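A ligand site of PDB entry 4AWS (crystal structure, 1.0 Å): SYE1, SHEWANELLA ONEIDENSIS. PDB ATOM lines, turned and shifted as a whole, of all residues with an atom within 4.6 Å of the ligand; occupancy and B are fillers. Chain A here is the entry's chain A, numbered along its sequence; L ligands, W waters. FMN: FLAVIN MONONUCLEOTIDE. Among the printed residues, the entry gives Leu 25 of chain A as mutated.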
ATOM      1  N   PRO A  23     -22.822  -7.640   0.370  1.00  0.00           N
ATOM      2  CA  PRO A  23     -22.500  -9.019  -0.044  1.00  0.00           C
ATOM      3  C   PRO A  23     -20.997  -9.264   0.153  1.00  0.00           C
ATOM      4  O   PRO A  23     -20.242  -8.319   0.418  1.00  0.00           O
ATOM      5  CB  PRO A  23     -22.880  -9.018  -1.518  1.00  0.00           C
ATOM      6  CG  PRO A  23     -22.500  -7.632  -1.972  1.00  0.00           C
ATOM      7  CD  PRO A  23     -22.813  -6.732  -0.796  1.00  0.00           C
ATOM      8  N   PRO A  24     -20.588 -10.509   0.014  1.00  0.00           N
ATOM      9  CA  PRO A  24     -19.157 -10.838   0.177  1.00  0.00           C
ATOM     10  C   PRO A  24     -18.295 -10.096  -0.813  1.00  0.00           C
ATOM     11  O   PRO A  24     -18.568 -10.116  -2.016  1.00  0.00           O
ATOM     12  CB  PRO A  24     -19.105 -12.336  -0.115  1.00  0.00           C
ATOM     13  CG  PRO A  24     -20.440 -12.789   0.313  1.00  0.00           C
ATOM     14  CD  PRO A  24     -21.398 -11.723  -0.207  1.00  0.00           C
ATOM     15  N   LEU A  25     -17.218  -9.487  -0.315  1.00  0.00           N
ATOM     16  CA  LEU A  25     -16.283  -8.743  -1.165  1.00  0.00           C
ATOM     17  C   LEU A  25     -14.847  -9.028  -0.701  1.00  0.00           C
ATOM     18  O   LEU A  25     -14.342  -8.419   0.236  1.00  0.00           O
ATOM     19  CB  LEU A  25     -16.546  -7.245  -1.115  1.00  0.00           C
ATOM     20  CG  LEU A  25     -17.946  -6.834  -1.607  1.00  0.00           C
ATOM     21  CD1 LEU A  25     -18.343  -5.483  -0.970  1.00  0.00           C
ATOM     22  CD2 LEU A  25     -17.984  -6.817  -3.134  1.00  0.00           C
ATOM     23  N   THR A  26     -14.194  -9.955  -1.401  1.00  0.00           N
ATOM     24  CA  THR A  26     -12.760 -10.209  -1.171  1.00  0.00           C
ATOM     25  C   THR A  26     -11.959  -8.925  -1.340  1.00  0.00           C
ATOM     26  O   THR A  26     -12.031  -8.295  -2.380  1.00  0.00           O
ATOM     27  CB  THR A  26     -12.319 -11.249  -2.209  1.00  0.00           C
ATOM     28  OG1 THR A  26     -12.856 -12.537  -1.886  1.00  0.00           O
ATOM     29  CG2 THR A  26     -10.802 -11.431  -2.280  1.00  0.00           C
ATOM     30  N   GLU A  57     -16.455 -11.228   3.183  1.00  0.00           N
ATOM     31  CA  GLU A  57     -15.640 -11.787   2.111  1.00  0.00           C
ATOM     32  C   GLU A  57     -15.473 -13.279   2.336  1.00  0.00           C
ATOM     33  O   GLU A  57     -15.430 -13.781   3.451  1.00  0.00           O
ATOM     34  CB  GLU A  57     -14.299 -11.084   2.081  1.00  0.00           C
ATOM     35  CG  GLU A  57     -13.391 -11.258   3.288  1.00  0.00           C
ATOM     36  CD  GLU A  57     -12.510 -10.005   3.378  1.00  0.00           C
ATOM     37  OE1 GLU A  57     -11.567  -9.810   2.556  1.00  0.00           O
ATOM     38  OE2 GLU A  57     -12.749  -9.162   4.267  1.00  0.00           O
ATOM     39  N   GLY A  58     -15.256 -13.992   1.213  1.00  0.00           N
ATOM     40  CA  GLY A  58     -14.965 -15.409   1.357  1.00  0.00           C
ATOM     41  C   GLY A  58     -13.795 -15.637   2.289  1.00  0.00           C
ATOM     42  O   GLY A  58     -12.762 -14.980   2.244  1.00  0.00           O
ATOM     43  N   GLN A 100     -18.786 -15.960   5.099  1.00  0.00           N
ATOM     44  CA  GLN A 100     -18.887 -16.735   3.870  1.00  0.00           C
ATOM     45  C   GLN A 100     -17.816 -17.786   3.831  1.00  0.00           C
ATOM     46  O   GLN A 100     -16.634 -17.507   3.616  1.00  0.00           O
ATOM     47  CB  GLN A 100     -18.849 -15.872   2.617  1.00  0.00           C
ATOM     48  CG  GLN A 100     -19.134 -16.742   1.403  1.00  0.00           C
ATOM     49  CD  GLN A 100     -18.910 -16.091   0.075  1.00  0.00           C
ATOM     50  OE1 GLN A 100     -17.791 -15.679  -0.251  1.00  0.00           O
ATOM     51  NE2 GLN A 100     -19.954 -16.029  -0.750  1.00  0.00           N
ATOM     52  N   TRP A 102     -15.580 -20.577   2.345  1.00  0.00           N
ATOM     53  CA  TRP A 102     -15.069 -20.675   0.985  1.00  0.00           C
ATOM     54  C   TRP A 102     -14.189 -21.912   0.783  1.00  0.00           C
ATOM     55  O   TRP A 102     -13.245 -22.129   1.515  1.00  0.00           O
ATOM     56  CB  TRP A 102     -14.225 -19.450   0.659  1.00  0.00           C
ATOM     57  CG  TRP A 102     -14.199 -19.025  -0.791  1.00  0.00           C
ATOM     58  CD1 TRP A 102     -14.842 -19.533  -1.881  1.00  0.00           C
ATOM     59  CD2 TRP A 102     -13.442 -17.894  -1.256  1.00  0.00           C
ATOM     60  NE1 TRP A 102     -14.552 -18.775  -2.992  1.00  0.00           N
ATOM     61  CE2 TRP A 102     -13.710 -17.756  -2.642  1.00  0.00           C
ATOM     62  CE3 TRP A 102     -12.596 -16.984  -0.631  1.00  0.00           C
ATOM     63  CZ2 TRP A 102     -13.165 -16.740  -3.396  1.00  0.00           C
ATOM     64  CZ3 TRP A 102     -12.066 -15.975  -1.398  1.00  0.00           C
ATOM     65  CH2 TRP A 102     -12.332 -15.853  -2.745  1.00  0.00           C
ATOM     66  N   HIS A 181     -20.503 -20.556   0.221  1.00  0.00           N
ATOM     67  CA  HIS A 181     -20.219 -20.089  -1.124  1.00  0.00           C
ATOM     68  C   HIS A 181     -20.343 -21.273  -2.081  1.00  0.00           C
ATOM     69  O   HIS A 181     -19.403 -22.071  -2.204  1.00  0.00           O
ATOM     70  CB  HIS A 181     -18.832 -19.436  -1.241  1.00  0.00           C
ATOM     71  CG  HIS A 181     -18.680 -18.636  -2.475  1.00  0.00           C
ATOM     72  ND1 HIS A 181     -19.543 -18.661  -3.531  1.00  0.00           N
ATOM     73  CD2 HIS A 181     -17.716 -17.680  -2.729  1.00  0.00           C
ATOM     74  CE1 HIS A 181     -19.105 -17.784  -4.395  1.00  0.00           C
ATOM     75  NE2 HIS A 181     -18.040 -17.155  -3.957  1.00  0.00           N
ATOM     76  N   ASN A 184     -20.219 -18.803  -8.165  1.00  0.00           N
ATOM     77  CA  ASN A 184     -19.154 -18.146  -8.892  1.00  0.00           C
ATOM     78  C   ASN A 184     -18.011 -19.101  -9.264  1.00  0.00           C
ATOM     79  O   ASN A 184     -16.850 -18.727  -9.285  1.00  0.00           O
ATOM     80  CB  ASN A 184     -18.678 -16.892  -8.169  1.00  0.00           C
ATOM     81  CG  ASN A 184     -19.798 -15.924  -7.986  1.00  0.00           C
ATOM     82  OD1 ASN A 184     -20.859 -16.024  -8.628  1.00  0.00           O
ATOM     83  ND2 ASN A 184     -19.625 -14.927  -7.110  1.00  0.00           N
ATOM     84  N   ARG A 233     -25.168 -19.347  -1.111  1.00  0.00           N
ATOM     85  CA  ARG A 233     -25.068 -18.542  -2.322  1.00  0.00           C
ATOM     86  C   ARG A 233     -24.931 -19.448  -3.555  1.00  0.00           C
ATOM     87  O   ARG A 233     -24.120 -20.362  -3.568  1.00  0.00           O
ATOM     88  CB  ARG A 233     -23.861 -17.572  -2.251  1.00  0.00           C
ATOM     89  CG  ARG A 233     -24.065 -16.384  -3.173  1.00  0.00           C
ATOM     90  CD  ARG A 233     -23.016 -15.296  -3.006  1.00  0.00           C
ATOM     91  NE  ARG A 233     -23.570 -14.042  -3.501  1.00  0.00           N
ATOM     92  CZ  ARG A 233     -22.881 -12.977  -3.889  1.00  0.00           C
ATOM     93  NH1 ARG A 233     -21.604 -13.016  -4.087  1.00  0.00           N
ATOM     94  NH2 ARG A 233     -23.544 -11.851  -4.179  1.00  0.00           N
ATOM     95  N   ALA A 270     -26.284 -14.728  -6.825  1.00  0.00           N
ATOM     96  CA  ALA A 270     -25.278 -13.859  -7.425  1.00  0.00           C
ATOM     97  C   ALA A 270     -25.629 -13.719  -8.894  1.00  0.00           C
ATOM     98  O   ALA A 270     -25.325 -14.586  -9.731  1.00  0.00           O
ATOM     99  CB  ALA A 270     -23.901 -14.436  -7.214  1.00  0.00           C
ATOM    100  N   VAL A 272     -24.975 -11.203 -11.111  1.00  0.00           N
ATOM    101  CA  VAL A 272     -23.908 -10.645 -11.944  1.00  0.00           C
ATOM    102  C   VAL A 272     -22.585 -11.008 -11.298  1.00  0.00           C
ATOM    103  O   VAL A 272     -22.500 -10.953 -10.050  1.00  0.00           O
ATOM    104  CB  VAL A 272     -24.004  -9.115 -12.078  1.00  0.00           C
ATOM    105  CG1 VAL A 272     -22.829  -8.535 -12.869  1.00  0.00           C
ATOM    106  CG2 VAL A 272     -25.346  -8.711 -12.693  1.00  0.00           C
ATOM    107  N   ASP A 273     -21.583 -11.316 -12.109  1.00  0.00           N
ATOM    108  CA  ASP A 273     -20.213 -11.479 -11.604  1.00  0.00           C
ATOM    109  C   ASP A 273     -19.338 -10.587 -12.467  1.00  0.00           C
ATOM    110  O   ASP A 273     -19.209 -10.862 -13.676  1.00  0.00           O
ATOM    111  CB  ASP A 273     -19.764 -12.931 -11.569  1.00  0.00           C
ATOM    112  CG  ASP A 273     -18.630 -13.136 -10.546  1.00  0.00           C
ATOM    113  OD1 ASP A 273     -18.615 -12.449  -9.429  1.00  0.00           O
ATOM    114  OD2 ASP A 273     -17.855 -14.050 -10.773  1.00  0.00           O
ATOM    115  N   TRP A 274     -18.841  -9.492 -11.935  1.00  0.00           N
ATOM    116  CA  TRP A 274     -18.010  -8.522 -12.666  1.00  0.00           C
ATOM    117  C   TRP A 274     -18.847  -7.939 -13.803  1.00  0.00           C
ATOM    118  O   TRP A 274     -19.823  -7.221 -13.551  1.00  0.00           O
ATOM    119  CB  TRP A 274     -16.639  -9.086 -13.036  1.00  0.00           C
ATOM    120  CG  TRP A 274     -15.902  -9.410 -11.785  1.00  0.00           C
ATOM    121  CD1 TRP A 274     -15.799 -10.601 -11.160  1.00  0.00           C
ATOM    122  CD2 TRP A 274     -15.148  -8.505 -10.962  1.00  0.00           C
ATOM    123  NE1 TRP A 274     -15.045 -10.517 -10.016  1.00  0.00           N
ATOM    124  CE2 TRP A 274     -14.642  -9.212  -9.885  1.00  0.00           C
ATOM    125  CE3 TRP A 274     -14.890  -7.141 -11.035  1.00  0.00           C
ATOM    126  CZ2 TRP A 274     -13.872  -8.662  -8.892  1.00  0.00           C
ATOM    127  CZ3 TRP A 274     -14.100  -6.563 -10.048  1.00  0.00           C
ATOM    128  CH2 TRP A 274     -13.612  -7.356  -8.999  1.00  0.00           C
ATOM    129  N   ALA A 299     -27.989 -10.115  -5.653  1.00  0.00           N
ATOM    130  CA  ALA A 299     -26.992  -9.064  -5.851  1.00  0.00           C
ATOM    131  C   ALA A 299     -26.523  -9.102  -7.290  1.00  0.00           C
ATOM    132  O   ALA A 299     -26.412 -10.174  -7.887  1.00  0.00           O
ATOM    133  CB  ALA A 299     -25.763  -9.275  -4.946  1.00  0.00           C
ATOM    134  N   GLY A 300     -26.222  -7.926  -7.815  1.00  0.00           N
ATOM    135  CA  GLY A 300     -25.616  -7.782  -9.138  1.00  0.00           C
ATOM    136  C   GLY A 300     -26.238  -6.620  -9.887  1.00  0.00           C
ATOM    137  O   GLY A 300     -27.346  -6.694 -10.381  1.00  0.00           O
ATOM    138  N   ARG A 301     -25.474  -5.523  -9.932  1.00  0.00           N
ATOM    139  CA  ARG A 301     -25.835  -4.311 -10.679  1.00  0.00           C
ATOM    140  C   ARG A 301     -27.166  -3.735 -10.247  1.00  0.00           C
ATOM    141  O   ARG A 301     -27.844  -3.057 -11.026  1.00  0.00           O
ATOM    142  CB  ARG A 301     -25.751  -4.452 -12.193  1.00  0.00           C
ATOM    143  CG  ARG A 301     -24.374  -4.791 -12.721  1.00  0.00           C
ATOM    144  CD  ARG A 301     -23.358  -3.711 -12.452  1.00  0.00           C
ATOM    145  NE  ARG A 301     -22.190  -3.881 -13.313  1.00  0.00           N
ATOM    146  CZ  ARG A 301     -21.022  -3.232 -13.062  1.00  0.00           C
ATOM    147  NH1 ARG A 301     -20.880  -2.461 -12.049  1.00  0.00           N
ATOM    148  NH2 ARG A 301     -20.066  -3.468 -13.939  1.00  0.00           N
ATOM    149  N   GLY A 320     -28.400  -7.106  -2.250  1.00  0.00           N
ATOM    150  CA  GLY A 320     -27.013  -6.777  -2.009  1.00  0.00           C
ATOM    151  C   GLY A 320     -26.473  -5.801  -3.036  1.00  0.00           C
ATOM    152  O   GLY A 320     -26.825  -5.867  -4.221  1.00  0.00           O
ATOM    153  N   PHE A 321     -25.587  -4.940  -2.555  1.00  0.00           N
ATOM    154  CA  PHE A 321     -24.889  -3.934  -3.379  1.00  0.00           C
ATOM    155  C   PHE A 321     -23.406  -4.143  -3.100  1.00  0.00           C
ATOM    156  O   PHE A 321     -22.971  -3.917  -1.979  1.00  0.00           O
ATOM    157  CB  PHE A 321     -25.293  -2.525  -3.001  1.00  0.00           C
ATOM    158  CG  PHE A 321     -26.770  -2.251  -3.132  1.00  0.00           C
ATOM    159  CD1 PHE A 321     -27.637  -2.596  -2.125  1.00  0.00           C
ATOM    160  CD2 PHE A 321     -27.275  -1.623  -4.247  1.00  0.00           C
ATOM    161  CE1 PHE A 321     -28.989  -2.345  -2.208  1.00  0.00           C
ATOM    162  CE2 PHE A 321     -28.661  -1.365  -4.344  1.00  0.00           C
ATOM    163  CZ  PHE A 321     -29.494  -1.716  -3.309  1.00  0.00           C
ATOM    164  N   GLY A 322     -22.663  -4.617  -4.075  1.00  0.00           N
ATOM    165  CA  GLY A 322     -21.244  -4.947  -3.883  1.00  0.00           C
ATOM    166  C   GLY A 322     -20.333  -3.761  -4.120  1.00  0.00           C
ATOM    167  O   GLY A 322     -19.898  -3.082  -3.191  1.00  0.00           O
ATOM    168  N   ARG A 323     -20.065  -3.493  -5.390  1.00  0.00           N
ATOM    169  CA  ARG A 323     -19.186  -2.378  -5.744  1.00  0.00           C
ATOM    170  C   ARG A 323     -19.607  -1.068  -5.107  1.00  0.00           C
ATOM    171  O   ARG A 323     -18.748  -0.340  -4.590  1.00  0.00           O
ATOM    172  CB  ARG A 323     -18.997  -2.344  -7.261  1.00  0.00           C
ATOM    173  CG  ARG A 323     -18.072  -3.490  -7.688  1.00  0.00           C
ATOM    174  CD  ARG A 323     -18.096  -3.815  -9.176  1.00  0.00           C
ATOM    175  NE  ARG A 323     -19.333  -4.560  -9.474  1.00  0.00           N
ATOM    176  CZ  ARG A 323     -19.510  -5.159 -10.633  1.00  0.00           C
ATOM    177  NH1 ARG A 323     -18.560  -5.066 -11.583  1.00  0.00           N
ATOM    178  NH2 ARG A 323     -20.602  -5.856 -10.880  1.00  0.00           N
ATOM    179  N   PRO A 324     -20.913  -0.718  -5.056  1.00  0.00           N
ATOM    180  CA  PRO A 324     -21.246   0.544  -4.379  1.00  0.00           C
ATOM    181  C   PRO A 324     -20.882   0.550  -2.891  1.00  0.00           C
ATOM    182  O   PRO A 324     -20.575   1.632  -2.349  1.00  0.00           O
ATOM    183  CB  PRO A 324     -22.774   0.641  -4.581  1.00  0.00           C
ATOM    184  CG  PRO A 324     -22.991  -0.101  -5.889  1.00  0.00           C
ATOM    185  CD  PRO A 324     -22.066  -1.281  -5.794  1.00  0.00           C
ATOM    186  N   ILE A 326     -18.253  -0.752  -1.546  1.00  0.00           N
ATOM    187  CA  ILE A 326     -16.816  -0.525  -1.398  1.00  0.00           C
ATOM    188  C   ILE A 326     -16.550   0.971  -1.234  1.00  0.00           C
ATOM    189  O   ILE A 326     -15.803   1.360  -0.337  1.00  0.00           O
ATOM    190  CB  ILE A 326     -16.056  -1.110  -2.585  1.00  0.00           C
ATOM    191  CG1 ILE A 326     -16.225  -2.641  -2.554  1.00  0.00           C
ATOM    192  CG2 ILE A 326     -14.620  -0.678  -2.655  1.00  0.00           C
ATOM    193  CD1 ILE A 326     -15.610  -3.290  -3.768  1.00  0.00           C
ATOM    194  N   LEU A 349      -8.786  -2.519  -4.934  1.00  0.00           N
ATOM    195  CA  LEU A 349      -9.707  -3.573  -4.502  1.00  0.00           C
ATOM    196  C   LEU A 349      -8.999  -4.643  -3.692  1.00  0.00           C
ATOM    197  O   LEU A 349      -9.557  -5.103  -2.680  1.00  0.00           O
ATOM    198  CB  LEU A 349     -10.393  -4.208  -5.700  1.00  0.00           C
ATOM    199  CG  LEU A 349     -11.467  -3.316  -6.330  1.00  0.00           C
ATOM    200  CD1 LEU A 349     -11.962  -3.959  -7.606  1.00  0.00           C
ATOM    201  CD2 LEU A 349     -12.603  -3.036  -5.374  1.00  0.00           C
ATOM    202  N   PHE A 350      -7.809  -5.062  -4.099  1.00  0.00           N
ATOM    203  CA  PHE A 350      -7.133  -6.205  -3.577  1.00  0.00           C
ATOM    204  C   PHE A 350      -5.747  -5.861  -3.073  1.00  0.00           C
ATOM    205  O   PHE A 350      -4.930  -5.270  -3.808  1.00  0.00           O
ATOM    206  CB  PHE A 350      -6.980  -7.307  -4.644  1.00  0.00           C
ATOM    207  CG  PHE A 350      -8.295  -7.679  -5.290  1.00  0.00           C
ATOM    208  CD1 PHE A 350      -9.323  -8.230  -4.581  1.00  0.00           C
ATOM    209  CD2 PHE A 350      -8.499  -7.405  -6.628  1.00  0.00           C
ATOM    210  CE1 PHE A 350     -10.492  -8.556  -5.190  1.00  0.00           C
ATOM    211  CE2 PHE A 350      -9.714  -7.660  -7.225  1.00  0.00           C
ATOM    212  CZ  PHE A 350     -10.693  -8.291  -6.527  1.00  0.00           C
HETATM  213  N1  FMN L   1     -18.678 -12.796  -4.215  1.00  0.00           N
HETATM  214  C2  FMN L   1     -18.587 -13.816  -3.337  1.00  0.00           C
HETATM  215  O2  FMN L   1     -19.501 -14.663  -3.195  1.00  0.00           O
HETATM  216  N3  FMN L   1     -17.481 -13.912  -2.530  1.00  0.00           N
HETATM  217  C4  FMN L   1     -16.427 -13.018  -2.535  1.00  0.00           C
HETATM  218  O4  FMN L   1     -15.511 -13.144  -1.694  1.00  0.00           O
HETATM  219  C4A FMN L   1     -16.497 -12.028  -3.531  1.00  0.00           C
HETATM  220  N5  FMN L   1     -15.467 -11.113  -3.631  1.00  0.00           N
HETATM  221  C5A FMN L   1     -15.666 -10.027  -4.458  1.00  0.00           C
HETATM  222  C6  FMN L   1     -14.730  -9.020  -4.503  1.00  0.00           C
HETATM  223  C7  FMN L   1     -14.897  -7.845  -5.238  1.00  0.00           C
HETATM  224  C7M FMN L   1     -13.873  -6.740  -5.116  1.00  0.00           C
HETATM  225  C8  FMN L   1     -16.044  -7.705  -6.007  1.00  0.00           C
HETATM  226  C8M FMN L   1     -16.295  -6.466  -6.762  1.00  0.00           C
HETATM  227  C9  FMN L   1     -17.019  -8.720  -5.994  1.00  0.00           C
HETATM  228  C9A FMN L   1     -16.840  -9.898  -5.238  1.00  0.00           C
HETATM  229  N10 FMN L   1     -17.834 -10.876  -5.144  1.00  0.00           N
HETATM  230  C10 FMN L   1     -17.688 -11.934  -4.291  1.00  0.00           C
HETATM  231  C1' FMN L   1     -19.126 -10.651  -5.863  1.00  0.00           C
HETATM  232  C2' FMN L   1     -20.030  -9.699  -5.121  1.00  0.00           C
HETATM  233  O2' FMN L   1     -20.523 -10.245  -3.897  1.00  0.00           O
HETATM  234  C3' FMN L   1     -21.253  -9.306  -5.954  1.00  0.00           C
HETATM  235  O3' FMN L   1     -22.107 -10.446  -6.149  1.00  0.00           O
HETATM  236  C4' FMN L   1     -20.968  -8.689  -7.301  1.00  0.00           C
HETATM  237  O4' FMN L   1     -19.925  -7.687  -7.193  1.00  0.00           O
HETATM  238  C5' FMN L   1     -22.198  -8.151  -7.999  1.00  0.00           C
HETATM  239  O5' FMN L   1     -22.810  -7.103  -7.234  1.00  0.00           O
HETATM  240  P   FMN L   1     -22.533  -5.534  -7.641  1.00  0.00           P
HETATM  241  O1P FMN L   1     -21.082  -5.256  -7.315  1.00  0.00           O
HETATM  242  O2P FMN L   1     -22.812  -5.394  -9.140  1.00  0.00           O
HETATM  243  O3P FMN L   1     -23.493  -4.773  -6.752  1.00  0.00           O
HETATM  244  O   HOH W   1     -18.319  -8.391  -9.371  1.00  0.00           O
HETATM  245  O   HOH W   2     -17.210 -10.545  -8.681  1.00  0.00           O
HETATM  246  O   HOH W   3     -16.814 -14.839  -5.766  1.00  0.00           O
HETATM  247  O   HOH W   4     -24.600  -2.367  -7.703  1.00  0.00           O
HETATM  248  O   HOH W   5     -26.125  -5.306  -6.766  1.00  0.00           O
HETATM  249  O   HOH W   6     -16.616 -12.852  -7.488  1.00  0.00           O
HETATM  250  O   HOH W   7     -22.376  -2.704  -9.807  1.00  0.00           O
HETATM  251  O   HOH W   8     -21.072 -12.221  -8.050  1.00  0.00           O
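Residues that only touch the ligand: Pro 23, Leu 25, Asn 184, Val 272, Trp 274, Gly 300, Phe 321, Pro 324, Leu 349 and Phe 350.
Hydrophobic or aromatic side chains within 4 Å of the ligand: Pro 23, Pro 24, Leu 25, His 181, Trp 274, Pro 324, Leu 349 and Phe 350.
The backbone carbonyl oxygen (O) of Trp 274 lies within hydrogen-bond range of the guanidinium group (NH2) of Arg 323, 3.1 Å away.
OE1 of Gln 100 sits close to N of Gly 58 (3.4 Å).
O2' of the ligand is in hydrogen-bond range of O of Pro 24 (2.7 Å).
N of Thr 26 is in hydrogen-bond range of N5 of the ligand (2.8 Å).
O4 of the ligand sits at hydrogen-bond distance from OG1 of Thr 26 (2.7 Å).
The backbone NH of Arg 301 sits at hydrogen-bond distance from an oxygen (O2P) of the ligand, 2.8 Å away.
O1P of the ligand sits at hydrogen-bond distance from N of Arg 323 (2.8 Å).
The guanidinium group of Arg 323 is in salt-bridge range of an oxygen (O2P) of the ligand (2.9 Å).
The backbone NH of Gly 322 is in hydrogen-bond range of an oxygen (O3P) of the ligand (2.8 Å).
An oxygen (O3') of the ligand sits at hydrogen-bond distance from the guanidinium group of Arg 233.
The side-chain amide nitrogen (NE2) of Gln 100 sits at hydrogen-bond distance from an oxygen (O2) of the ligand.
A ring nitrogen (NE2) of His 181 sits at hydrogen-bond distance from an oxygen (O2) of the ligand.
The backbone NH (N) of Gly 58 sits at hydrogen-bond distance from an oxygen (O4) of the ligand, 3.0 Å away.
Water W5 lies within hydrogen-bond range of an oxygen (O3P) of the ligand (2.7 Å), the backbone carbonyl oxygen of Gly 320 (2.7 Å), the backbone NH of Gly 300 (2.8 Å) and the backbone NH of Arg 301 (3.2 Å).
Water W1 lies within hydrogen-bond range of an oxygen (O4') of the ligand (2.8 Å) and the backbone NH (N) of Trp 274 (2.8 Å).
Water W8 lies within hydrogen-bond range of O of Val 272, O3' of the ligand, OD1 of Asp 273 and ND2 of Asn 184.
Water W7 lies within hydrogen-bond range of the guanidinium group (NH1) of Arg 301 and an oxygen (O2P) of the ligand.
Water W3 lies within hydrogen-bond range of ND2 of Asn 184, N1 of the ligand and NE2 of His 181.
Water W2 lies within hydrogen-bond range of the side-chain carboxylate of Asp 273 (2.5 Å) and the indole nitrogen of Trp 274 (2.5 Å).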
